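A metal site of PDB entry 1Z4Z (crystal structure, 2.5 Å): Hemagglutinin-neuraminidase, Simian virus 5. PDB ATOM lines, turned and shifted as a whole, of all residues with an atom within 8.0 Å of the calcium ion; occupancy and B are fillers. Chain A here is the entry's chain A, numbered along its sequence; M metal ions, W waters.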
ATOM      1  N   GLN A 212      18.435   1.528  -1.800  1.00  0.00           N
ATOM      2  CA  GLN A 212      19.858   1.808  -1.906  1.00  0.00           C
ATOM      3  C   GLN A 212      20.290   1.593  -3.350  1.00  0.00           C
ATOM      4  O   GLN A 212      19.564   0.982  -4.137  1.00  0.00           O
ATOM      5  CB  GLN A 212      20.618   0.846  -1.008  1.00  0.00           C
ATOM      6  CG  GLN A 212      20.499  -0.608  -1.442  1.00  0.00           C
ATOM      7  CD  GLN A 212      21.043  -1.562  -0.409  1.00  0.00           C
ATOM      8  OE1 GLN A 212      21.939  -1.223   0.348  1.00  0.00           O
ATOM      9  NE2 GLN A 212      20.506  -2.782  -0.393  1.00  0.00           N
ATOM     10  N   GLU A 214      21.640   0.230  -6.791  1.00  0.00           N
ATOM     11  CA  GLU A 214      21.572  -1.123  -7.337  1.00  0.00           C
ATOM     12  C   GLU A 214      22.755  -1.987  -6.943  1.00  0.00           C
ATOM     13  O   GLU A 214      22.584  -3.125  -6.499  1.00  0.00           O
ATOM     14  CB  GLU A 214      21.466  -1.071  -8.861  1.00  0.00           C
ATOM     15  CG  GLU A 214      21.609  -2.433  -9.525  1.00  0.00           C
ATOM     16  CD  GLU A 214      21.307  -2.398 -11.006  1.00  0.00           C
ATOM     17  OE1 GLU A 214      21.804  -1.478 -11.686  1.00  0.00           O
ATOM     18  OE2 GLU A 214      20.583  -3.294 -11.491  1.00  0.00           O
ATOM     19  N   ARG A 215      23.957  -1.455  -7.119  1.00  0.00           N
ATOM     20  CA  ARG A 215      25.146  -2.220  -6.797  1.00  0.00           C
ATOM     21  C   ARG A 215      25.137  -2.716  -5.346  1.00  0.00           C
ATOM     22  O   ARG A 215      25.539  -3.844  -5.059  1.00  0.00           O
ATOM     23  CB  ARG A 215      26.398  -1.396  -7.064  1.00  0.00           C
ATOM     24  CG  ARG A 215      27.645  -2.228  -7.061  1.00  0.00           C
ATOM     25  CD  ARG A 215      28.878  -1.378  -7.204  1.00  0.00           C
ATOM     26  NE  ARG A 215      30.073  -2.203  -7.046  1.00  0.00           N
ATOM     27  CZ  ARG A 215      31.257  -1.727  -6.664  1.00  0.00           C
ATOM     28  NH1 ARG A 215      31.384  -0.432  -6.400  1.00  0.00           N
ATOM     29  NH2 ARG A 215      32.284  -2.548  -6.533  1.00  0.00           N
ATOM     30  N   ASP A 216      24.652  -1.876  -4.440  1.00  0.00           N
ATOM     31  CA  ASP A 216      24.598  -2.245  -3.028  1.00  0.00           C
ATOM     32  C   ASP A 216      23.674  -3.434  -2.816  1.00  0.00           C
ATOM     33  O   ASP A 216      23.895  -4.250  -1.912  1.00  0.00           O
ATOM     34  CB  ASP A 216      24.117  -1.072  -2.176  1.00  0.00           C
ATOM     35  CG  ASP A 216      25.068   0.115  -2.235  1.00  0.00           C
ATOM     36  OD1 ASP A 216      26.124   0.002  -2.884  1.00  0.00           O
ATOM     37  OD2 ASP A 216      24.758   1.165  -1.642  1.00  0.00           O
ATOM     38  N   ASP A 217      22.638  -3.556  -3.647  1.00  0.00           N
ATOM     39  CA  ASP A 217      21.722  -4.677  -3.516  1.00  0.00           C
ATOM     40  C   ASP A 217      22.451  -5.998  -3.764  1.00  0.00           C
ATOM     41  O   ASP A 217      22.107  -7.005  -3.184  1.00  0.00           O
ATOM     42  CB  ASP A 217      20.556  -4.578  -4.503  1.00  0.00           C
ATOM     43  CG  ASP A 217      19.486  -3.612  -4.039  1.00  0.00           C
ATOM     44  OD1 ASP A 217      19.212  -3.575  -2.821  1.00  0.00           O
ATOM     45  OD2 ASP A 217      18.903  -2.914  -4.895  1.00  0.00           O
ATOM     46  N   TYR A 218      23.449  -6.005  -4.635  1.00  0.00           N
ATOM     47  CA  TYR A 218      24.156  -7.249  -4.887  1.00  0.00           C
ATOM     48  C   TYR A 218      25.121  -7.648  -3.770  1.00  0.00           C
ATOM     49  O   TYR A 218      25.337  -8.839  -3.525  1.00  0.00           O
ATOM     50  CB  TYR A 218      24.913  -7.171  -6.217  1.00  0.00           C
ATOM     51  CG  TYR A 218      23.999  -7.224  -7.409  1.00  0.00           C
ATOM     52  CD1 TYR A 218      23.302  -6.100  -7.838  1.00  0.00           C
ATOM     53  CD2 TYR A 218      23.783  -8.424  -8.095  1.00  0.00           C
ATOM     54  CE1 TYR A 218      22.406  -6.162  -8.902  1.00  0.00           C
ATOM     55  CE2 TYR A 218      22.887  -8.503  -9.155  1.00  0.00           C
ATOM     56  CZ  TYR A 218      22.197  -7.364  -9.553  1.00  0.00           C
ATOM     57  OH  TYR A 218      21.286  -7.434 -10.579  1.00  0.00           O
ATOM     58  N   PHE A 219      25.703  -6.665  -3.087  1.00  0.00           N
ATOM     59  CA  PHE A 219      26.621  -6.961  -1.995  1.00  0.00           C
ATOM     60  C   PHE A 219      25.898  -7.393  -0.734  1.00  0.00           C
ATOM     61  O   PHE A 219      26.377  -8.276  -0.027  1.00  0.00           O
ATOM     62  CB  PHE A 219      27.507  -5.750  -1.700  1.00  0.00           C
ATOM     63  CG  PHE A 219      28.638  -5.598  -2.672  1.00  0.00           C
ATOM     64  CD1 PHE A 219      28.451  -4.946  -3.878  1.00  0.00           C
ATOM     65  CD2 PHE A 219      29.884  -6.156  -2.399  1.00  0.00           C
ATOM     66  CE1 PHE A 219      29.488  -4.857  -4.809  1.00  0.00           C
ATOM     67  CE2 PHE A 219      30.920  -6.083  -3.326  1.00  0.00           C
ATOM     68  CZ  PHE A 219      30.719  -5.432  -4.534  1.00  0.00           C
ATOM     69  N   SER A 220      24.748  -6.781  -0.446  1.00  0.00           N
ATOM     70  CA  SER A 220      23.997  -7.167   0.736  1.00  0.00           C
ATOM     71  C   SER A 220      23.464  -8.581   0.529  1.00  0.00           C
ATOM     72  O   SER A 220      22.957  -8.905  -0.544  1.00  0.00           O
ATOM     73  CB  SER A 220      22.865  -6.171   1.006  1.00  0.00           C
ATOM     74  OG  SER A 220      21.970  -6.060  -0.079  1.00  0.00           O
ATOM     75  N   ALA A 221      23.615  -9.428   1.534  1.00  0.00           N
ATOM     76  CA  ALA A 221      23.143 -10.803   1.420  1.00  0.00           C
ATOM     77  C   ALA A 221      21.624 -10.904   1.445  1.00  0.00           C
ATOM     78  O   ALA A 221      21.052 -11.881   0.965  1.00  0.00           O
ATOM     79  CB  ALA A 221      23.729 -11.637   2.554  1.00  0.00           C
ATOM     80  N   ALA A 222      20.981  -9.891   2.009  1.00  0.00           N
ATOM     81  CA  ALA A 222      19.523  -9.878   2.085  1.00  0.00           C
ATOM     82  C   ALA A 222      18.946  -9.283   0.814  1.00  0.00           C
ATOM     83  O   ALA A 222      19.420  -8.277   0.343  1.00  0.00           O
ATOM     84  CB  ALA A 222      19.073  -9.047   3.282  1.00  0.00           C
ATOM     85  N   PRO A 223      17.890  -9.878   0.270  1.00  0.00           N
ATOM     86  CA  PRO A 223      17.257  -9.390  -0.962  1.00  0.00           C
ATOM     87  C   PRO A 223      16.263  -8.270  -0.671  1.00  0.00           C
ATOM     88  O   PRO A 223      15.756  -8.163   0.442  1.00  0.00           O
ATOM     89  CB  PRO A 223      16.571 -10.629  -1.497  1.00  0.00           C
ATOM     90  CG  PRO A 223      16.082 -11.267  -0.236  1.00  0.00           C
ATOM     91  CD  PRO A 223      17.271 -11.148   0.696  1.00  0.00           C
ATOM     92  N   PRO A 224      15.980  -7.411  -1.672  1.00  0.00           N
ATOM     93  CA  PRO A 224      15.025  -6.319  -1.464  1.00  0.00           C
ATOM     94  C   PRO A 224      13.628  -6.894  -1.248  1.00  0.00           C
ATOM     95  O   PRO A 224      13.358  -8.039  -1.598  1.00  0.00           O
ATOM     96  CB  PRO A 224      15.102  -5.536  -2.772  1.00  0.00           C
ATOM     97  CG  PRO A 224      16.433  -5.892  -3.333  1.00  0.00           C
ATOM     98  CD  PRO A 224      16.555  -7.345  -3.028  1.00  0.00           C
ATOM     99  N   TRP A 251      19.285 -15.633  -3.198  1.00  0.00           N
ATOM    100  CA  TRP A 251      19.434 -14.476  -4.070  1.00  0.00           C
ATOM    101  C   TRP A 251      19.799 -13.239  -3.268  1.00  0.00           C
ATOM    102  O   TRP A 251      19.086 -12.850  -2.338  1.00  0.00           O
ATOM    103  CB  TRP A 251      18.117 -14.203  -4.824  1.00  0.00           C
ATOM    104  CG  TRP A 251      17.701 -15.277  -5.788  1.00  0.00           C
ATOM    105  CD1 TRP A 251      17.293 -16.555  -5.480  1.00  0.00           C
ATOM    106  CD2 TRP A 251      17.606 -15.166  -7.222  1.00  0.00           C
ATOM    107  NE1 TRP A 251      16.951 -17.237  -6.622  1.00  0.00           N
ATOM    108  CE2 TRP A 251      17.139 -16.410  -7.702  1.00  0.00           C
ATOM    109  CE3 TRP A 251      17.878 -14.141  -8.127  1.00  0.00           C
ATOM    110  CZ2 TRP A 251      16.928 -16.648  -9.070  1.00  0.00           C
ATOM    111  CZ3 TRP A 251      17.666 -14.371  -9.489  1.00  0.00           C
ATOM    112  CH2 TRP A 251      17.194 -15.625  -9.942  1.00  0.00           C
ATOM    113  N   ALA A 252      20.917 -12.615  -3.606  1.00  0.00           N
ATOM    114  CA  ALA A 252      21.327 -11.397  -2.915  1.00  0.00           C
ATOM    115  C   ALA A 252      20.365 -10.311  -3.389  1.00  0.00           C
ATOM    116  O   ALA A 252      20.057  -9.402  -2.654  1.00  0.00           O
ATOM    117  CB  ALA A 252      22.782 -11.049  -3.257  1.00  0.00           C
ATOM    118  N   THR A 253      19.870 -10.417  -4.613  1.00  0.00           N
ATOM    119  CA  THR A 253      18.909  -9.447  -5.120  1.00  0.00           C
ATOM    120  C   THR A 253      17.987 -10.158  -6.066  1.00  0.00           C
ATOM    121  O   THR A 253      18.332 -11.211  -6.617  1.00  0.00           O
ATOM    122  CB  THR A 253      19.541  -8.326  -5.952  1.00  0.00           C
ATOM    123  OG1 THR A 253      20.916  -8.190  -5.589  1.00  0.00           O
ATOM    124  CG2 THR A 253      18.810  -7.014  -5.693  1.00  0.00           C
ATOM    125  N   LEU A 254      16.804  -9.575  -6.260  1.00  0.00           N
ATOM    126  CA  LEU A 254      15.796 -10.121  -7.157  1.00  0.00           C
ATOM    127  C   LEU A 254      15.041  -8.938  -7.735  1.00  0.00           C
ATOM    128  O   LEU A 254      14.610  -8.054  -6.997  1.00  0.00           O
ATOM    129  CB  LEU A 254      14.863 -11.055  -6.381  1.00  0.00           C
ATOM    130  CG  LEU A 254      13.776 -11.793  -7.156  1.00  0.00           C
ATOM    131  CD1 LEU A 254      14.377 -12.573  -8.318  1.00  0.00           C
ATOM    132  CD2 LEU A 254      13.047 -12.738  -6.211  1.00  0.00           C
ATOM    133  N   GLY A 275      21.086 -11.560  -8.624  1.00  0.00           N
ATOM    134  CA  GLY A 275      22.361 -12.183  -8.345  1.00  0.00           C
ATOM    135  C   GLY A 275      22.238 -13.295  -7.316  1.00  0.00           C
ATOM    136  O   GLY A 275      21.652 -13.113  -6.248  1.00  0.00           O
ATOM    137  N   ILE A 277      23.893 -16.122  -4.687  1.00  0.00           N
ATOM    138  CA  ILE A 277      25.008 -16.272  -3.762  1.00  0.00           C
ATOM    139  C   ILE A 277      25.825 -17.530  -3.987  1.00  0.00           C
ATOM    140  O   ILE A 277      25.280 -18.615  -4.234  1.00  0.00           O
ATOM    141  CB  ILE A 277      24.479 -16.256  -2.318  1.00  0.00           C
ATOM    142  CG1 ILE A 277      23.862 -14.890  -2.021  1.00  0.00           C
ATOM    143  CG2 ILE A 277      25.595 -16.602  -1.345  1.00  0.00           C
ATOM    144  CD1 ILE A 277      23.158 -14.812  -0.678  1.00  0.00           C
ATOM    145  N   ARG A 323      28.285 -12.052  -7.540  1.00  0.00           N
ATOM    146  CA  ARG A 323      27.124 -12.908  -7.613  1.00  0.00           C
ATOM    147  C   ARG A 323      26.983 -13.501  -9.008  1.00  0.00           C
ATOM    148  O   ARG A 323      27.559 -13.006  -9.980  1.00  0.00           O
ATOM    149  CB  ARG A 323      25.847 -12.116  -7.318  1.00  0.00           C
ATOM    150  CG  ARG A 323      25.897 -11.268  -6.061  1.00  0.00           C
ATOM    151  CD  ARG A 323      26.141 -12.108  -4.836  1.00  0.00           C
ATOM    152  NE  ARG A 323      26.033 -11.325  -3.617  1.00  0.00           N
ATOM    153  CZ  ARG A 323      26.400 -11.761  -2.428  1.00  0.00           C
ATOM    154  NH1 ARG A 323      26.895 -12.995  -2.308  1.00  0.00           N
ATOM    155  NH2 ARG A 323      26.266 -10.991  -1.357  1.00  0.00           N
HETATM  156 CA    CA M   1      20.863  -7.739  -1.350  1.00  0.00          CA
HETATM  157  O   HOH W   1      18.859  -5.390  -0.952  1.00  0.00           O
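Merely in contact with the calcium ion: Pro 223 (3.98 Å).
Of the 19 residues printed, 5 come within 4 Å of the calcium ion.
The calcium ion is bound by the backbone carbonyl oxygen (O) of Ala 252 (2.3 Å), the backbone carbonyl oxygen (O) of Ala 222 (2.3 Å), the backbone carbonyl oxygen (O) of Asp 217 (2.3 Å), the side-chain hydroxyl (OG) of Ser 220 (2.4 Å) and the backbone carbonyl oxygen (O) of Ser 220 (2.5 Å).
Slightly farther from the calcium ion lies water W1 (3.1 Å).
Water W1 lies within hydrogen-bond range of OD1 of Asp 217 (2.6 Å) and NE2 of Gln 212 (3.1 Å).
N of Ala 252 sits at hydrogen-bond distance from O of Gly 275, 2.8 Å away.
O of Asp 217 lies close to OG1 of Thr 253, 2.9 Å away.
The side-chain carboxylate (OD1) of Asp 217 sits at hydrogen-bond distance from the side-chain amide nitrogen (NE2) of Gln 212 (2.9 Å).
The side-chain hydroxyl of Ser 220 sits close to the backbone carbonyl oxygen of Asp 216 (3.2 Å).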
